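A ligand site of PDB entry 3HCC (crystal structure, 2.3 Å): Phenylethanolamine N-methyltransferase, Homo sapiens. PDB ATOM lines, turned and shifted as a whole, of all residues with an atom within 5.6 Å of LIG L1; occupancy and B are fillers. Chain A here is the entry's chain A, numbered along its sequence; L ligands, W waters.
OH of Tyr 40 sits at hydrogen-bond distance from O1 of LIG L1 (2.6 Å).
O2 of LIG L1 is in hydrogen-bond range of OH of Tyr 85, 2.6 Å away.
The side-chain hydroxyl of Tyr 35 sits at hydrogen-bond distance from an oxygen (O1) of LIG L1 (2.7 Å).
The backbone carbonyl oxygen of Ala 181 sits at hydrogen-bond distance from a nitrogen (N1) of LIG L1 (2.8 Å).
O4 of LIG L1 is in hydrogen-bond range of ND2 of Asn 106, at 2.8 Å.
The backbone carbonyl oxygen (O) of Gly 79 sits at hydrogen-bond distance from a nitrogen (N1) of LIG L1, 2.9 Å away.
An oxygen (O4) of LIG L1 is in hydrogen-bond range of the side-chain carboxylate (OD1) of Asp 101 (3.0 Å).
N of Val 159 is in hydrogen-bond range of N5 of LIG L1, at 3.0 Å.
The backbone carbonyl oxygen of Ser 80 lies close to a nitrogen (N1) of LIG L1 (3.1 Å).
The side-chain carboxylate (OD1) of Asp 158 lies within hydrogen-bond range of a nitrogen (N4) of LIG L1, at 3.2 Å.
The side-chain sulfur (SG) of Cys 183 sits at hydrogen-bond distance from a nitrogen (N6) of LIG L1.
O of Phe 182 sits close to S1 of LIG L1, at 3.7 Å.
Residues that only touch LIG L1: Tyr 27, Gly 81, Thr 83, Gln 86, Phe 102, Leu 103, Ile 157, His 160 and Val 187.
Of the 28 residues printed, 21 come within 4 Å of LIG L1.
The nearest printed residue that does not touch LIG L1 is Tyr 222 (4.1 Å).
OD2 of Asp 101 sits at hydrogen-bond distance from ND2 of Asn 106 (2.7 Å).
N of Gly 81 lies within hydrogen-bond range of OD1 of Asp 101 (3.1 Å).
The backbone NH (N) of Leu 103 is in hydrogen-bond range of the side-chain carboxylate (OD2) of Asp 101 (3.2 Å).
O of Ser 80 is in hydrogen-bond range of NE2 of Gln 86, at 3.4 Å.
OG1 of Thr 83 lies within hydrogen-bond range of OE1 of Gln 86 (2.7 Å).
A ring nitrogen (NE2) of His 160 is in hydrogen-bond range of the backbone carbonyl oxygen (O) of Val 187, 3.0 Å away.
OH of Tyr 27 is in hydrogen-bond range of O of Ala 186 (2.6 Å).
OD2 of Asp 77 is in hydrogen-bond range of NE2 of Gln 86 (2.8 Å).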
ATOM      1  N   TYR A  27      -5.878  25.985 -13.293  1.00  0.00           N
ATOM      2  CA  TYR A  27      -7.164  25.976 -12.605  1.00  0.00           C
ATOM      3  C   TYR A  27      -8.080  27.122 -13.037  1.00  0.00           C
ATOM      4  O   TYR A  27      -9.216  27.223 -12.582  1.00  0.00           O
ATOM      5  CB  TYR A  27      -6.966  25.952 -11.083  1.00  0.00           C
ATOM      6  CG  TYR A  27      -6.773  24.551 -10.550  1.00  0.00           C
ATOM      7  CD1 TYR A  27      -5.511  24.081 -10.233  1.00  0.00           C
ATOM      8  CD2 TYR A  27      -7.850  23.704 -10.395  1.00  0.00           C
ATOM      9  CE1 TYR A  27      -5.337  22.792  -9.755  1.00  0.00           C
ATOM     10  CE2 TYR A  27      -7.688  22.415  -9.925  1.00  0.00           C
ATOM     11  CZ  TYR A  27      -6.422  21.964  -9.599  1.00  0.00           C
ATOM     12  OH  TYR A  27      -6.275  20.684  -9.131  1.00  0.00           O
ATOM     13  N   PHE A  30     -10.772  25.640 -15.242  1.00  0.00           N
ATOM     14  CA  PHE A  30     -11.538  24.642 -14.504  1.00  0.00           C
ATOM     15  C   PHE A  30     -13.034  24.918 -14.581  1.00  0.00           C
ATOM     16  O   PHE A  30     -13.496  25.988 -14.182  1.00  0.00           O
ATOM     17  CB  PHE A  30     -11.080  24.662 -13.037  1.00  0.00           C
ATOM     18  CG  PHE A  30     -11.722  23.631 -12.167  1.00  0.00           C
ATOM     19  CD1 PHE A  30     -11.134  22.381 -11.988  1.00  0.00           C
ATOM     20  CD2 PHE A  30     -12.893  23.913 -11.485  1.00  0.00           C
ATOM     21  CE1 PHE A  30     -11.720  21.439 -11.171  1.00  0.00           C
ATOM     22  CE2 PHE A  30     -13.488  22.967 -10.667  1.00  0.00           C
ATOM     23  CZ  PHE A  30     -12.896  21.730 -10.507  1.00  0.00           C
ATOM     24  N   TYR A  35     -16.564  19.129 -13.955  1.00  0.00           N
ATOM     25  CA  TYR A  35     -15.964  18.376 -12.865  1.00  0.00           C
ATOM     26  C   TYR A  35     -17.025  17.564 -12.109  1.00  0.00           C
ATOM     27  O   TYR A  35     -16.848  16.372 -11.872  1.00  0.00           O
ATOM     28  CB  TYR A  35     -15.223  19.317 -11.918  1.00  0.00           C
ATOM     29  CG  TYR A  35     -14.617  18.623 -10.720  1.00  0.00           C
ATOM     30  CD1 TYR A  35     -13.382  17.980 -10.803  1.00  0.00           C
ATOM     31  CD2 TYR A  35     -15.277  18.608  -9.494  1.00  0.00           C
ATOM     32  CE1 TYR A  35     -12.825  17.354  -9.708  1.00  0.00           C
ATOM     33  CE2 TYR A  35     -14.726  17.974  -8.389  1.00  0.00           C
ATOM     34  CZ  TYR A  35     -13.502  17.348  -8.507  1.00  0.00           C
ATOM     35  OH  TYR A  35     -12.954  16.718  -7.411  1.00  0.00           O
ATOM     36  N   TYR A  40     -19.144  12.968 -10.136  1.00  0.00           N
ATOM     37  CA  TYR A  40     -20.244  12.880  -9.183  1.00  0.00           C
ATOM     38  C   TYR A  40     -21.586  12.570  -9.839  1.00  0.00           C
ATOM     39  O   TYR A  40     -22.630  12.645  -9.204  1.00  0.00           O
ATOM     40  CB  TYR A  40     -20.255  14.142  -8.316  1.00  0.00           C
ATOM     41  CG  TYR A  40     -19.001  14.211  -7.477  1.00  0.00           C
ATOM     42  CD1 TYR A  40     -17.902  14.980  -7.874  1.00  0.00           C
ATOM     43  CD2 TYR A  40     -18.875  13.456  -6.329  1.00  0.00           C
ATOM     44  CE1 TYR A  40     -16.748  15.012  -7.116  1.00  0.00           C
ATOM     45  CE2 TYR A  40     -17.728  13.476  -5.575  1.00  0.00           C
ATOM     46  CZ  TYR A  40     -16.665  14.254  -5.968  1.00  0.00           C
ATOM     47  OH  TYR A  40     -15.533  14.265  -5.190  1.00  0.00           O
ATOM     48  N   LYS A  57     -16.067   6.358  -0.001  1.00  0.00           N
ATOM     49  CA  LYS A  57     -15.718   7.623   0.635  1.00  0.00           C
ATOM     50  C   LYS A  57     -16.680   7.967   1.770  1.00  0.00           C
ATOM     51  O   LYS A  57     -16.248   8.308   2.872  1.00  0.00           O
ATOM     52  CB  LYS A  57     -15.675   8.748  -0.392  1.00  0.00           C
ATOM     53  CG  LYS A  57     -14.524   8.631  -1.380  1.00  0.00           C
ATOM     54  CD  LYS A  57     -14.376   9.882  -2.226  1.00  0.00           C
ATOM     55  CE  LYS A  57     -15.501  10.016  -3.222  1.00  0.00           C
ATOM     56  NZ  LYS A  57     -15.395  11.279  -3.992  1.00  0.00           N
ATOM     57  N   ASP A  77     -13.253  22.959   5.893  1.00  0.00           N
ATOM     58  CA  ASP A  77     -13.094  22.086   4.736  1.00  0.00           C
ATOM     59  C   ASP A  77     -12.221  22.768   3.694  1.00  0.00           C
ATOM     60  O   ASP A  77     -12.583  23.821   3.167  1.00  0.00           O
ATOM     61  CB  ASP A  77     -14.463  21.746   4.132  1.00  0.00           C
ATOM     62  CG  ASP A  77     -14.363  20.848   2.921  1.00  0.00           C
ATOM     63  OD1 ASP A  77     -13.438  20.015   2.859  1.00  0.00           O
ATOM     64  OD2 ASP A  77     -15.230  20.958   2.021  1.00  0.00           O
ATOM     65  N   ILE A  78     -11.065  22.166   3.412  1.00  0.00           N
ATOM     66  CA  ILE A  78     -10.033  22.771   2.574  1.00  0.00           C
ATOM     67  C   ILE A  78     -10.144  22.346   1.117  1.00  0.00           C
ATOM     68  O   ILE A  78     -10.044  21.169   0.796  1.00  0.00           O
ATOM     69  CB  ILE A  78      -8.628  22.360   3.063  1.00  0.00           C
ATOM     70  CG1 ILE A  78      -8.500  22.576   4.573  1.00  0.00           C
ATOM     71  CG2 ILE A  78      -7.559  23.124   2.292  1.00  0.00           C
ATOM     72  CD1 ILE A  78      -8.677  24.007   4.996  1.00  0.00           C
ATOM     73  N   GLY A  79     -10.321  23.328   0.234  1.00  0.00           N
ATOM     74  CA  GLY A  79     -10.421  23.037  -1.194  1.00  0.00           C
ATOM     75  C   GLY A  79     -11.706  22.303  -1.498  1.00  0.00           C
ATOM     76  O   GLY A  79     -11.696  21.246  -2.137  1.00  0.00           O
ATOM     77  N   SER A  80     -12.819  22.868  -1.028  1.00  0.00           N
ATOM     78  CA  SER A  80     -14.134  22.264  -1.179  1.00  0.00           C
ATOM     79  C   SER A  80     -14.489  22.003  -2.632  1.00  0.00           C
ATOM     80  O   SER A  80     -15.170  21.023  -2.948  1.00  0.00           O
ATOM     81  CB  SER A  80     -15.197  23.177  -0.563  1.00  0.00           C
ATOM     82  OG  SER A  80     -14.997  23.327   0.835  1.00  0.00           O
ATOM     83  N   GLY A  81     -14.035  22.884  -3.509  1.00  0.00           N
ATOM     84  CA  GLY A  81     -14.457  22.849  -4.889  1.00  0.00           C
ATOM     85  C   GLY A  81     -15.949  23.121  -4.936  1.00  0.00           C
ATOM     86  O   GLY A  81     -16.462  23.884  -4.120  1.00  0.00           O
ATOM     87  N   PRO A  82     -16.653  22.502  -5.887  1.00  0.00           N
ATOM     88  CA  PRO A  82     -18.112  22.635  -5.988  1.00  0.00           C
ATOM     89  C   PRO A  82     -18.882  21.510  -5.288  1.00  0.00           C
ATOM     90  O   PRO A  82     -20.078  21.349  -5.532  1.00  0.00           O
ATOM     91  CB  PRO A  82     -18.322  22.560  -7.497  1.00  0.00           C
ATOM     92  CG  PRO A  82     -17.332  21.502  -7.897  1.00  0.00           C
ATOM     93  CD  PRO A  82     -16.087  21.890  -7.105  1.00  0.00           C
ATOM     94  N   THR A  83     -18.226  20.759  -4.410  1.00  0.00           N
ATOM     95  CA  THR A  83     -18.864  19.592  -3.781  1.00  0.00           C
ATOM     96  C   THR A  83     -19.131  19.785  -2.292  1.00  0.00           C
ATOM     97  O   THR A  83     -18.443  20.563  -1.616  1.00  0.00           O
ATOM     98  CB  THR A  83     -18.033  18.310  -3.967  1.00  0.00           C
ATOM     99  OG1 THR A  83     -16.896  18.353  -3.095  1.00  0.00           O
ATOM    100  CG2 THR A  83     -17.558  18.178  -5.407  1.00  0.00           C
ATOM    101  N   TYR A  85     -20.447  16.733  -0.476  1.00  0.00           N
ATOM    102  CA  TYR A  85     -20.544  15.371   0.035  1.00  0.00           C
ATOM    103  C   TYR A  85     -19.561  15.111   1.173  1.00  0.00           C
ATOM    104  O   TYR A  85     -19.842  14.316   2.076  1.00  0.00           O
ATOM    105  CB  TYR A  85     -20.279  14.357  -1.086  1.00  0.00           C
ATOM    106  CG  TYR A  85     -18.812  14.197  -1.403  1.00  0.00           C
ATOM    107  CD1 TYR A  85     -18.034  13.275  -0.715  1.00  0.00           C
ATOM    108  CD2 TYR A  85     -18.193  14.978  -2.378  1.00  0.00           C
ATOM    109  CE1 TYR A  85     -16.689  13.130  -0.989  1.00  0.00           C
ATOM    110  CE2 TYR A  85     -16.850  14.837  -2.661  1.00  0.00           C
ATOM    111  CZ  TYR A  85     -16.101  13.907  -1.957  1.00  0.00           C
ATOM    112  OH  TYR A  85     -14.765  13.758  -2.230  1.00  0.00           O
ATOM    113  N   GLN A  86     -18.406  15.772   1.133  1.00  0.00           N
ATOM    114  CA  GLN A  86     -17.362  15.517   2.117  1.00  0.00           C
ATOM    115  C   GLN A  86     -17.735  15.970   3.535  1.00  0.00           C
ATOM    116  O   GLN A  86     -16.974  15.758   4.474  1.00  0.00           O
ATOM    117  CB  GLN A  86     -16.023  16.126   1.686  1.00  0.00           C
ATOM    118  CG  GLN A  86     -16.001  17.642   1.561  1.00  0.00           C
ATOM    119  CD  GLN A  86     -16.463  18.143   0.203  1.00  0.00           C
ATOM    120  OE1 GLN A  86     -17.123  17.413  -0.538  1.00  0.00           O
ATOM    121  NE2 GLN A  86     -16.119  19.373  -0.123  1.00  0.00           N
ATOM    122  N   ASP A 101     -12.327  27.506  -1.103  1.00  0.00           N
ATOM    123  CA  ASP A 101     -11.763  27.116  -2.385  1.00  0.00           C
ATOM    124  C   ASP A 101     -11.073  28.275  -3.092  1.00  0.00           C
ATOM    125  O   ASP A 101     -11.382  29.438  -2.854  1.00  0.00           O
ATOM    126  CB  ASP A 101     -12.826  26.525  -3.319  1.00  0.00           C
ATOM    127  CG  ASP A 101     -12.202  25.719  -4.443  1.00  0.00           C
ATOM    128  OD1 ASP A 101     -11.607  24.660  -4.150  1.00  0.00           O
ATOM    129  OD2 ASP A 101     -12.301  26.151  -5.608  1.00  0.00           O
ATOM    130  N   PHE A 102     -10.144  27.932  -3.963  1.00  0.00           N
ATOM    131  CA  PHE A 102      -9.299  28.879  -4.669  1.00  0.00           C
ATOM    132  C   PHE A 102     -10.068  29.648  -5.747  1.00  0.00           C
ATOM    133  O   PHE A 102      -9.742  30.796  -6.050  1.00  0.00           O
ATOM    134  CB  PHE A 102      -8.121  28.130  -5.284  1.00  0.00           C
ATOM    135  CG  PHE A 102      -7.079  29.010  -5.920  1.00  0.00           C
ATOM    136  CD1 PHE A 102      -6.215  29.759  -5.127  1.00  0.00           C
ATOM    137  CD2 PHE A 102      -6.940  29.068  -7.294  1.00  0.00           C
ATOM    138  CE1 PHE A 102      -5.246  30.566  -5.708  1.00  0.00           C
ATOM    139  CE2 PHE A 102      -5.971  29.876  -7.875  1.00  0.00           C
ATOM    140  CZ  PHE A 102      -5.126  30.617  -7.080  1.00  0.00           C
ATOM    141  N   LEU A 103     -11.089  29.010  -6.312  1.00  0.00           N
ATOM    142  CA  LEU A 103     -11.809  29.574  -7.447  1.00  0.00           C
ATOM    143  C   LEU A 103     -13.144  30.207  -7.063  1.00  0.00           C
ATOM    144  O   LEU A 103     -13.933  29.626  -6.319  1.00  0.00           O
ATOM    145  CB  LEU A 103     -12.041  28.509  -8.526  1.00  0.00           C
ATOM    146  CG  LEU A 103     -10.814  27.911  -9.219  1.00  0.00           C
ATOM    147  CD1 LEU A 103     -11.248  26.850 -10.225  1.00  0.00           C
ATOM    148  CD2 LEU A 103      -9.994  28.997  -9.907  1.00  0.00           C
ATOM    149  N   ASN A 106     -16.161  28.118  -8.075  1.00  0.00           N
ATOM    150  CA  ASN A 106     -16.496  27.042  -7.145  1.00  0.00           C
ATOM    151  C   ASN A 106     -17.284  27.557  -5.942  1.00  0.00           C
ATOM    152  O   ASN A 106     -18.277  26.952  -5.530  1.00  0.00           O
ATOM    153  CB  ASN A 106     -15.239  26.304  -6.693  1.00  0.00           C
ATOM    154  CG  ASN A 106     -14.734  25.332  -7.737  1.00  0.00           C
ATOM    155  OD1 ASN A 106     -15.519  24.720  -8.463  1.00  0.00           O
ATOM    156  ND2 ASN A 106     -13.412  25.177  -7.824  1.00  0.00           N
ATOM    157  N   ILE A 157      -9.324  30.541  -0.532  1.00  0.00           N
ATOM    158  CA  ILE A 157      -8.179  29.929   0.131  1.00  0.00           C
ATOM    159  C   ILE A 157      -7.099  29.613  -0.876  1.00  0.00           C
ATOM    160  O   ILE A 157      -7.374  29.376  -2.054  1.00  0.00           O
ATOM    161  CB  ILE A 157      -8.580  28.633   0.856  1.00  0.00           C
ATOM    162  CG1 ILE A 157      -7.429  28.128   1.731  1.00  0.00           C
ATOM    163  CG2 ILE A 157      -8.999  27.563  -0.147  1.00  0.00           C
ATOM    164  CD1 ILE A 157      -7.742  26.866   2.494  1.00  0.00           C
ATOM    165  N   ASP A 158      -5.853  29.623  -0.410  1.00  0.00           N
ATOM    166  CA  ASP A 158      -4.716  29.217  -1.212  1.00  0.00           C
ATOM    167  C   ASP A 158      -3.769  28.426  -0.314  1.00  0.00           C
ATOM    168  O   ASP A 158      -3.098  29.002   0.544  1.00  0.00           O
ATOM    169  CB  ASP A 158      -4.017  30.427  -1.815  1.00  0.00           C
ATOM    170  CG  ASP A 158      -2.843  30.042  -2.710  1.00  0.00           C
ATOM    171  OD1 ASP A 158      -2.273  28.943  -2.509  1.00  0.00           O
ATOM    172  OD2 ASP A 158      -2.496  30.835  -3.610  1.00  0.00           O
ATOM    173  N   VAL A 159      -3.724  27.121  -0.520  1.00  0.00           N
ATOM    174  CA  VAL A 159      -2.940  26.245   0.338  1.00  0.00           C
ATOM    175  C   VAL A 159      -1.438  26.507   0.218  1.00  0.00           C
ATOM    176  O   VAL A 159      -0.662  26.084   1.072  1.00  0.00           O
ATOM    177  CB  VAL A 159      -3.220  24.761   0.048  1.00  0.00           C
ATOM    178  CG1 VAL A 159      -4.694  24.456   0.277  1.00  0.00           C
ATOM    179  CG2 VAL A 159      -2.820  24.422  -1.380  1.00  0.00           C
ATOM    180  N   HIS A 160      -1.044  27.212  -0.831  1.00  0.00           N
ATOM    181  CA  HIS A 160       0.372  27.497  -1.064  1.00  0.00           C
ATOM    182  C   HIS A 160       0.903  28.616  -0.174  1.00  0.00           C
ATOM    183  O   HIS A 160       2.115  28.749   0.005  1.00  0.00           O
ATOM    184  CB  HIS A 160       0.611  27.808  -2.551  1.00  0.00           C
ATOM    185  CG  HIS A 160       0.290  26.678  -3.474  1.00  0.00           C
ATOM    186  ND1 HIS A 160       0.846  25.421  -3.324  1.00  0.00           N
ATOM    187  CD2 HIS A 160      -0.507  26.610  -4.563  1.00  0.00           C
ATOM    188  CE1 HIS A 160       0.389  24.629  -4.283  1.00  0.00           C
ATOM    189  NE2 HIS A 160      -0.433  25.333  -5.042  1.00  0.00           N
ATOM    190  N   ALA A 181     -10.575  17.034   0.622  1.00  0.00           N
ATOM    191  CA  ALA A 181     -10.707  15.940  -0.327  1.00  0.00           C
ATOM    192  C   ALA A 181     -10.204  16.317  -1.721  1.00  0.00           C
ATOM    193  O   ALA A 181     -10.724  17.233  -2.361  1.00  0.00           O
ATOM    194  CB  ALA A 181     -12.158  15.468  -0.395  1.00  0.00           C
ATOM    195  N   PHE A 182      -9.188  15.599  -2.180  1.00  0.00           N
ATOM    196  CA  PHE A 182      -8.638  15.770  -3.528  1.00  0.00           C
ATOM    197  C   PHE A 182      -8.111  17.171  -3.801  1.00  0.00           C
ATOM    198  O   PHE A 182      -8.217  17.676  -4.928  1.00  0.00           O
ATOM    199  CB  PHE A 182      -9.679  15.388  -4.572  1.00  0.00           C
ATOM    200  CG  PHE A 182     -10.201  14.001  -4.421  1.00  0.00           C
ATOM    201  CD1 PHE A 182     -11.451  13.776  -3.861  1.00  0.00           C
ATOM    202  CD2 PHE A 182      -9.438  12.916  -4.813  1.00  0.00           C
ATOM    203  CE1 PHE A 182     -11.928  12.490  -3.707  1.00  0.00           C
ATOM    204  CE2 PHE A 182      -9.915  11.630  -4.659  1.00  0.00           C
ATOM    205  CZ  PHE A 182     -11.159  11.413  -4.109  1.00  0.00           C
ATOM    206  N   CYS A 183      -7.542  17.812  -2.788  1.00  0.00           N
ATOM    207  CA  CYS A 183      -7.028  19.167  -2.931  1.00  0.00           C
ATOM    208  C   CYS A 183      -5.497  19.228  -3.066  1.00  0.00           C
ATOM    209  O   CYS A 183      -4.972  19.652  -4.097  1.00  0.00           O
ATOM    210  CB  CYS A 183      -7.480  20.038  -1.768  1.00  0.00           C
ATOM    211  SG  CYS A 183      -6.989  21.777  -1.933  1.00  0.00           S
ATOM    212  N   ALA A 186      -3.688  17.583  -5.912  1.00  0.00           N
ATOM    213  CA  ALA A 186      -4.220  18.145  -7.150  1.00  0.00           C
ATOM    214  C   ALA A 186      -3.708  19.554  -7.427  1.00  0.00           C
ATOM    215  O   ALA A 186      -3.872  20.073  -8.530  1.00  0.00           O
ATOM    216  CB  ALA A 186      -5.748  18.130  -7.131  1.00  0.00           C
ATOM    217  N   VAL A 187      -3.085  20.167  -6.433  1.00  0.00           N
ATOM    218  CA  VAL A 187      -2.576  21.533  -6.579  1.00  0.00           C
ATOM    219  C   VAL A 187      -1.063  21.627  -6.393  1.00  0.00           C
ATOM    220  O   VAL A 187      -0.493  22.721  -6.415  1.00  0.00           O
ATOM    221  CB  VAL A 187      -3.269  22.498  -5.598  1.00  0.00           C
ATOM    222  CG1 VAL A 187      -4.778  22.487  -5.837  1.00  0.00           C
ATOM    223  CG2 VAL A 187      -2.949  22.118  -4.161  1.00  0.00           C
ATOM    224  N   TYR A 222      -6.136  15.038 -14.435  1.00  0.00           N
ATOM    225  CA  TYR A 222      -7.562  14.816 -14.618  1.00  0.00           C
ATOM    226  C   TYR A 222      -8.127  15.989 -15.407  1.00  0.00           C
ATOM    227  O   TYR A 222      -7.533  17.070 -15.454  1.00  0.00           O
ATOM    228  CB  TYR A 222      -8.278  14.649 -13.277  1.00  0.00           C
ATOM    229  CG  TYR A 222      -8.393  15.914 -12.458  1.00  0.00           C
ATOM    230  CD1 TYR A 222      -9.517  16.725 -12.544  1.00  0.00           C
ATOM    231  CD2 TYR A 222      -7.374  16.311 -11.596  1.00  0.00           C
ATOM    232  CE1 TYR A 222      -9.626  17.880 -11.804  1.00  0.00           C
ATOM    233  CE2 TYR A 222      -7.470  17.466 -10.848  1.00  0.00           C
ATOM    234  CZ  TYR A 222      -8.604  18.244 -10.947  1.00  0.00           C
ATOM    235  OH  TYR A 222      -8.724  19.400 -10.215  1.00  0.00           O
HETATM  236  N1  LIG L   1     -13.079  18.732  -2.597  1.00  0.00           N
HETATM  237  C1  LIG L   1     -13.788  18.452  -3.829  1.00  0.00           C
HETATM  238  C2  LIG L   1     -13.132  19.121  -5.043  1.00  0.00           C
HETATM  239  C3  LIG L   1     -11.644  18.816  -5.208  1.00  0.00           C
HETATM  240  S1  LIG L   1     -10.960  19.420  -6.785  1.00  0.00           S
HETATM  241  C4  LIG L   1     -13.951  16.944  -4.028  1.00  0.00           C
HETATM  242  O1  LIG L   1     -14.339  16.585  -5.093  1.00  0.00           O
HETATM  243  O2  LIG L   1     -13.944  16.163  -2.869  1.00  0.00           O
HETATM  244  C5  LIG L   1      -9.553  20.454  -6.254  1.00  0.00           C
HETATM  245  C6  LIG L   1      -9.894  21.906  -5.864  1.00  0.00           C
HETATM  246  O3  LIG L   1      -8.730  22.531  -5.475  1.00  0.00           O
HETATM  247  C7  LIG L   1     -10.413  22.736  -7.032  1.00  0.00           C
HETATM  248  O4  LIG L   1     -11.710  23.186  -6.726  1.00  0.00           O
HETATM  249  C8  LIG L   1      -9.507  23.766  -7.127  1.00  0.00           C
HETATM  250  O5  LIG L   1     -10.072  24.994  -7.520  1.00  0.00           O
HETATM  251  C9  LIG L   1      -8.886  23.851  -5.850  1.00  0.00           C
HETATM  252  N2  LIG L   1      -7.618  24.569  -5.815  1.00  0.00           N
HETATM  253  C10 LIG L   1      -6.828  24.857  -6.842  1.00  0.00           C
HETATM  254  N3  LIG L   1      -5.721  25.531  -6.365  1.00  0.00           N
HETATM  255  C11 LIG L   1      -5.845  25.644  -5.003  1.00  0.00           C
HETATM  256  C12 LIG L   1      -5.049  26.224  -4.053  1.00  0.00           C
HETATM  257  N4  LIG L   1      -3.800  26.851  -4.426  1.00  0.00           N
HETATM  258  N5  LIG L   1      -5.415  26.193  -2.784  1.00  0.00           N
HETATM  259  C13 LIG L   1      -6.572  25.606  -2.419  1.00  0.00           C
HETATM  260  N6  LIG L   1      -7.362  25.037  -3.364  1.00  0.00           N
HETATM  261  C14 LIG L   1      -6.996  25.065  -4.648  1.00  0.00           C
HETATM  262  C1  LG2 L   2     -10.859  14.332  -8.585  1.00  0.00           C
HETATM  263  N1  LG2 L   2      -8.339  14.331  -8.802  1.00  0.00           N
HETATM  264  C2  LG2 L   2     -10.039  12.897 -10.273  1.00  0.00           C
HETATM  265  C3  LG2 L   2     -11.996  10.943  -7.726  1.00  0.00           C
HETATM  266  C4  LG2 L   2     -13.220  11.084  -7.086  1.00  0.00           C
HETATM  267  C5  LG2 L   2     -11.858  13.349  -7.954  1.00  0.00           C
HETATM  268  C6  LG2 L   2     -10.938  14.131 -10.090  1.00  0.00           C
HETATM  269  C7  LG2 L   2      -9.985  12.339  -8.868  1.00  0.00           C
HETATM  270  C8  LG2 L   2      -9.547  13.700  -8.235  1.00  0.00           C
HETATM  271  C9  LG2 L   2     -11.317  12.078  -8.176  1.00  0.00           C
HETATM  272  C10 LG2 L   2     -13.759  12.347  -6.892  1.00  0.00           C
HETATM  273  C11 LG2 L   2     -13.090  13.482  -7.327  1.00  0.00           C
HETATM  274  C12 LG2 L   2     -11.383   9.556  -7.934  1.00  0.00           C
HETATM  275  F1  LG2 L   2     -11.045   9.420  -9.208  1.00  0.00           F
HETATM  276  F2  LG2 L   2     -12.275   8.616  -7.614  1.00  0.00           F
HETATM  277  F3  LG2 L   2     -10.309   9.442  -7.166  1.00  0.00           F
HETATM  278  O   HOH W   1     -12.430  19.283   0.262  1.00  0.00           O
